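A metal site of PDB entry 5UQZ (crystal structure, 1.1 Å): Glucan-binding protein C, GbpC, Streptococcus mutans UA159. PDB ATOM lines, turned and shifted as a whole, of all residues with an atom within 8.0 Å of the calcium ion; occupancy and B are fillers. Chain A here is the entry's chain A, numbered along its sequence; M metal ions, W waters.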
ATOM      1  N   SER A 223     -18.932  24.575  25.499  1.00  0.00           N
ATOM      2  CA  SER A 223     -18.251  23.375  25.077  1.00  0.00           C
ATOM      3  C   SER A 223     -19.023  22.120  25.486  1.00  0.00           C
ATOM      4  O   SER A 223     -20.003  22.171  26.240  1.00  0.00           O
ATOM      5  CB  SER A 223     -16.869  23.341  25.702  1.00  0.00           C
ATOM      6  OG  SER A 223     -16.106  24.478  25.305  1.00  0.00           O
ATOM      7  N   SER A 224     -18.562  20.977  24.973  1.00  0.00           N
ATOM      8  CA  SER A 224     -19.017  19.696  25.467  1.00  0.00           C
ATOM      9  C   SER A 224     -20.547  19.527  25.320  1.00  0.00           C
ATOM     10  O   SER A 224     -21.252  19.060  26.204  1.00  0.00           O
ATOM     11  CB  SER A 224     -18.578  19.500  26.919  1.00  0.00           C
ATOM     12  OG  SER A 224     -18.853  18.196  27.385  1.00  0.00           O
ATOM     13  N   LEU A 225     -21.052  19.838  24.110  1.00  0.00           N
ATOM     14  CA  LEU A 225     -22.473  19.627  23.825  1.00  0.00           C
ATOM     15  C   LEU A 225     -22.619  18.271  23.153  1.00  0.00           C
ATOM     16  O   LEU A 225     -22.762  18.145  21.923  1.00  0.00           O
ATOM     17  CB  LEU A 225     -23.055  20.771  23.005  1.00  0.00           C
ATOM     18  CG  LEU A 225     -23.015  22.151  23.707  1.00  0.00           C
ATOM     19  CD1 LEU A 225     -23.582  23.206  22.793  1.00  0.00           C
ATOM     20  CD2 LEU A 225     -23.712  22.158  25.050  1.00  0.00           C
ATOM     21  N   ASN A 226     -22.629  17.238  23.990  1.00  0.00           N
ATOM     22  CA  ASN A 226     -22.640  15.874  23.464  1.00  0.00           C
ATOM     23  C   ASN A 226     -23.994  15.494  22.860  1.00  0.00           C
ATOM     24  O   ASN A 226     -25.036  15.839  23.424  1.00  0.00           O
ATOM     25  CB  ASN A 226     -22.377  14.859  24.595  1.00  0.00           C
ATOM     26  CG  ASN A 226     -21.097  15.142  25.339  1.00  0.00           C
ATOM     27  OD1 ASN A 226     -21.034  16.131  26.060  1.00  0.00           O
ATOM     28  ND2 ASN A 226     -20.064  14.330  25.130  1.00  0.00           N
ATOM     29  N   HIS A 227     -23.935  14.734  21.769  1.00  0.00           N
ATOM     30  CA  HIS A 227     -25.104  14.065  21.243  1.00  0.00           C
ATOM     31  C   HIS A 227     -24.658  12.633  20.978  1.00  0.00           C
ATOM     32  O   HIS A 227     -23.824  12.375  20.109  1.00  0.00           O
ATOM     33  CB  HIS A 227     -25.562  14.732  19.946  1.00  0.00           C
ATOM     34  CG  HIS A 227     -26.795  14.129  19.342  1.00  0.00           C
ATOM     35  ND1 HIS A 227     -27.477  14.715  18.291  1.00  0.00           N
ATOM     36  CD2 HIS A 227     -27.480  12.991  19.648  1.00  0.00           C
ATOM     37  CE1 HIS A 227     -28.531  13.977  17.994  1.00  0.00           C
ATOM     38  NE2 HIS A 227     -28.554  12.924  18.794  1.00  0.00           N
ATOM     39  N   HIS A 235     -29.377  10.965  23.405  1.00  0.00           N
ATOM     40  CA  HIS A 235     -29.026  11.952  24.419  1.00  0.00           C
ATOM     41  C   HIS A 235     -28.448  13.183  23.735  1.00  0.00           C
ATOM     42  O   HIS A 235     -27.443  13.072  23.028  1.00  0.00           O
ATOM     43  CB  HIS A 235     -27.938  11.308  25.260  1.00  0.00           C
ATOM     44  CG  HIS A 235     -27.340  12.214  26.303  1.00  0.00           C
ATOM     45  ND1 HIS A 235     -27.607  12.064  27.648  1.00  0.00           N
ATOM     46  CD2 HIS A 235     -26.457  13.246  26.220  1.00  0.00           C
ATOM     47  CE1 HIS A 235     -26.875  12.925  28.344  1.00  0.00           C
ATOM     48  NE2 HIS A 235     -26.173  13.676  27.493  1.00  0.00           N
ATOM     49  N   GLU A 237     -27.445  17.406  24.265  1.00  0.00           N
ATOM     50  CA  GLU A 237     -27.211  18.585  25.098  1.00  0.00           C
ATOM     51  C   GLU A 237     -27.353  19.816  24.227  1.00  0.00           C
ATOM     52  O   GLU A 237     -26.765  19.889  23.136  1.00  0.00           O
ATOM     53  CB  GLU A 237     -25.835  18.472  25.750  1.00  0.00           C
ATOM     54  CG  GLU A 237     -25.782  17.230  26.632  1.00  0.00           C
ATOM     55  CD  GLU A 237     -24.468  16.845  27.251  1.00  0.00           C
ATOM     56  OE1 GLU A 237     -23.494  17.611  27.227  1.00  0.00           O
ATOM     57  OE2 GLU A 237     -24.440  15.712  27.827  1.00  0.00           O
ATOM     58  N   GLN A 268     -20.522  11.613  19.150  1.00  0.00           N
ATOM     59  CA  GLN A 268     -19.811  10.877  20.201  1.00  0.00           C
ATOM     60  C   GLN A 268     -19.062   9.645  19.702  1.00  0.00           C
ATOM     61  O   GLN A 268     -18.019   9.305  20.285  1.00  0.00           O
ATOM     62  CB  GLN A 268     -20.837  10.392  21.250  1.00  0.00           C
ATOM     63  CG  GLN A 268     -20.196   9.904  22.540  1.00  0.00           C
ATOM     64  CD  GLN A 268     -19.758  11.049  23.456  1.00  0.00           C
ATOM     65  OE1 GLN A 268     -20.357  12.125  23.438  1.00  0.00           O
ATOM     66  NE2 GLN A 268     -18.719  10.838  24.246  1.00  0.00           N
ATOM     67  N   TRP A 284     -12.444  13.374  22.275  1.00  0.00           N
ATOM     68  CA  TRP A 284     -12.528  14.839  22.178  1.00  0.00           C
ATOM     69  C   TRP A 284     -13.108  15.467  23.439  1.00  0.00           C
ATOM     70  O   TRP A 284     -12.881  16.666  23.670  1.00  0.00           O
ATOM     71  CB  TRP A 284     -13.317  15.276  20.923  1.00  0.00           C
ATOM     72  CG  TRP A 284     -14.775  14.914  20.891  1.00  0.00           C
ATOM     73  CD1 TRP A 284     -15.335  13.903  20.175  1.00  0.00           C
ATOM     74  CD2 TRP A 284     -15.859  15.596  21.576  1.00  0.00           C
ATOM     75  NE1 TRP A 284     -16.703  13.875  20.401  1.00  0.00           N
ATOM     76  CE2 TRP A 284     -17.040  14.909  21.236  1.00  0.00           C
ATOM     77  CE3 TRP A 284     -15.955  16.715  22.416  1.00  0.00           C
ATOM     78  CZ2 TRP A 284     -18.272  15.293  21.737  1.00  0.00           C
ATOM     79  CZ3 TRP A 284     -17.153  17.084  22.913  1.00  0.00           C
ATOM     80  CH2 TRP A 284     -18.327  16.381  22.587  1.00  0.00           C
ATOM     81  N   ASP A 285     -13.859  14.715  24.248  1.00  0.00           N
ATOM     82  CA  ASP A 285     -14.574  15.256  25.403  1.00  0.00           C
ATOM     83  C   ASP A 285     -13.847  14.953  26.684  1.00  0.00           C
ATOM     84  O   ASP A 285     -14.405  15.192  27.754  1.00  0.00           O
ATOM     85  CB  ASP A 285     -16.001  14.697  25.430  1.00  0.00           C
ATOM     86  CG  ASP A 285     -16.921  15.491  26.354  1.00  0.00           C
ATOM     87  OD1 ASP A 285     -16.792  16.714  26.490  1.00  0.00           O
ATOM     88  OD2 ASP A 285     -17.822  14.837  26.956  1.00  0.00           O
ATOM     89  N   VAL A 287     -11.773  15.363  29.946  1.00  0.00           N
ATOM     90  CA  VAL A 287     -11.600  16.539  30.785  1.00  0.00           C
ATOM     91  C   VAL A 287     -10.817  16.161  32.032  1.00  0.00           C
ATOM     92  O   VAL A 287     -10.850  15.006  32.483  1.00  0.00           O
ATOM     93  CB  VAL A 287     -12.940  17.240  31.153  1.00  0.00           C
ATOM     94  CG1 VAL A 287     -13.683  17.697  29.892  1.00  0.00           C
ATOM     95  CG2 VAL A 287     -13.840  16.315  31.994  1.00  0.00           C
ATOM     96  N   GLY A 301     -16.976  19.400  19.676  1.00  0.00           N
ATOM     97  CA  GLY A 301     -18.236  19.349  20.374  1.00  0.00           C
ATOM     98  C   GLY A 301     -18.651  20.693  20.951  1.00  0.00           C
ATOM     99  O   GLY A 301     -19.505  20.719  21.837  1.00  0.00           O
ATOM    100  N   VAL A 316     -30.629  18.989  28.712  1.00  0.00           N
ATOM    101  CA  VAL A 316     -30.124  17.658  28.392  1.00  0.00           C
ATOM    102  C   VAL A 316     -31.280  16.694  28.515  1.00  0.00           C
ATOM    103  O   VAL A 316     -32.031  16.726  29.506  1.00  0.00           O
ATOM    104  CB  VAL A 316     -28.906  17.258  29.257  1.00  0.00           C
ATOM    105  CG1 VAL A 316     -29.197  17.364  30.763  1.00  0.00           C
ATOM    106  CG2 VAL A 316     -28.404  15.896  28.880  1.00  0.00           C
ATOM    107  N   THR A 326     -27.429  13.196  33.096  1.00  0.00           N
ATOM    108  CA  THR A 326     -26.457  14.095  33.726  1.00  0.00           C
ATOM    109  C   THR A 326     -25.884  15.044  32.700  1.00  0.00           C
ATOM    110  O   THR A 326     -25.808  14.715  31.516  1.00  0.00           O
ATOM    111  CB  THR A 326     -25.308  13.299  34.357  1.00  0.00           C
ATOM    112  OG1 THR A 326     -24.637  12.518  33.355  1.00  0.00           O
ATOM    113  CG2 THR A 326     -25.807  12.350  35.438  1.00  0.00           C
ATOM    114  N   ILE A 327     -25.367  16.171  33.185  1.00  0.00           N
ATOM    115  CA  ILE A 327     -24.547  17.072  32.391  1.00  0.00           C
ATOM    116  C   ILE A 327     -23.662  17.852  33.334  1.00  0.00           C
ATOM    117  O   ILE A 327     -24.127  18.362  34.381  1.00  0.00           O
ATOM    118  CB  ILE A 327     -25.404  18.009  31.506  1.00  0.00           C
ATOM    119  CG1 ILE A 327     -24.497  18.819  30.551  1.00  0.00           C
ATOM    120  CG2 ILE A 327     -26.313  18.906  32.300  1.00  0.00           C
ATOM    121  CD1 ILE A 327     -25.314  19.708  29.535  1.00  0.00           C
ATOM    122  N   TRP A 328     -22.393  18.022  32.947  1.00  0.00           N
ATOM    123  CA  TRP A 328     -21.507  18.978  33.590  1.00  0.00           C
ATOM    124  C   TRP A 328     -21.506  20.181  32.665  1.00  0.00           C
ATOM    125  O   TRP A 328     -20.875  20.151  31.600  1.00  0.00           O
ATOM    126  CB  TRP A 328     -20.102  18.437  33.766  1.00  0.00           C
ATOM    127  CG  TRP A 328     -19.180  19.383  34.473  1.00  0.00           C
ATOM    128  CD1 TRP A 328     -19.423  20.700  34.877  1.00  0.00           C
ATOM    129  CD2 TRP A 328     -17.882  19.069  34.946  1.00  0.00           C
ATOM    130  NE1 TRP A 328     -18.316  21.217  35.474  1.00  0.00           N
ATOM    131  CE2 TRP A 328     -17.365  20.243  35.550  1.00  0.00           C
ATOM    132  CE3 TRP A 328     -17.085  17.926  34.868  1.00  0.00           C
ATOM    133  CZ2 TRP A 328     -16.089  20.285  36.112  1.00  0.00           C
ATOM    134  CZ3 TRP A 328     -15.830  17.966  35.426  1.00  0.00           C
ATOM    135  CH2 TRP A 328     -15.345  19.151  36.042  1.00  0.00           C
ATOM    136  N   PHE A 329     -22.295  21.209  33.008  1.00  0.00           N
ATOM    137  CA  PHE A 329     -22.366  22.387  32.162  1.00  0.00           C
ATOM    138  C   PHE A 329     -21.469  23.437  32.772  1.00  0.00           C
ATOM    139  O   PHE A 329     -21.702  23.878  33.891  1.00  0.00           O
ATOM    140  CB  PHE A 329     -23.805  22.932  32.087  1.00  0.00           C
ATOM    141  CG  PHE A 329     -23.885  24.115  31.201  1.00  0.00           C
ATOM    142  CD1 PHE A 329     -23.996  23.958  29.827  1.00  0.00           C
ATOM    143  CD2 PHE A 329     -23.790  25.394  31.725  1.00  0.00           C
ATOM    144  CE1 PHE A 329     -23.989  25.088  28.995  1.00  0.00           C
ATOM    145  CE2 PHE A 329     -23.799  26.502  30.889  1.00  0.00           C
ATOM    146  CZ  PHE A 329     -23.909  26.350  29.527  1.00  0.00           C
ATOM    147  N   ALA A 330     -20.482  23.879  32.006  1.00  0.00           N
ATOM    148  CA  ALA A 330     -19.613  24.940  32.428  1.00  0.00           C
ATOM    149  C   ALA A 330     -19.596  26.005  31.346  1.00  0.00           C
ATOM    150  O   ALA A 330     -19.740  25.699  30.146  1.00  0.00           O
ATOM    151  CB  ALA A 330     -18.194  24.479  32.731  1.00  0.00           C
HETATM  152 CA    CA M   1     -21.133  17.490  27.962  1.00  0.00          CA
HETATM  153  O   HOH W   1     -22.156  15.288  28.790  1.00  0.00           O
HETATM  154  O   HOH W   2     -21.533  19.592  28.985  1.00  0.00           O
HETATM  155  O   HOH W   3     -21.063  17.112  30.410  1.00  0.00           O
HETATM  156  O   HOH W   4     -19.489  15.838  28.749  1.00  0.00           O
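N of Ser 224 is in hydrogen-bond range of O of Gly 301, 3.3 Å away.
The side-chain hydroxyl of Ser 224 lies close to the side-chain carboxylate of Asp 285 (2.7 Å).
The side-chain carboxylate (OE2) of Glu 237 sits at hydrogen-bond distance from a ring nitrogen (NE2) of His 235 (2.7 Å).
The side-chain amide oxygen (OE1) of Gln 268 sits at hydrogen-bond distance from the side-chain amide nitrogen (ND2) of Asn 226, at 2.8 Å.
The side-chain carboxylate (OD2) of Asp 285 sits at hydrogen-bond distance from the side-chain amide nitrogen (ND2) of Asn 226 (2.9 Å).
Three residues have an atom within 4 Å of the calcium ion: Ser 224, Asn 226 and Glu 237.
The nearest printed residue that does not touch the calcium ion is Asp 285 (4.4 Å).
The calcium ion is bound by OD1 of Asn 226, O of Ser 224, water W2, OG of Ser 224, water W4, OE1 of Glu 237, water W3 and water W1.
The calcium ion has eight donor atoms within binding distance.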
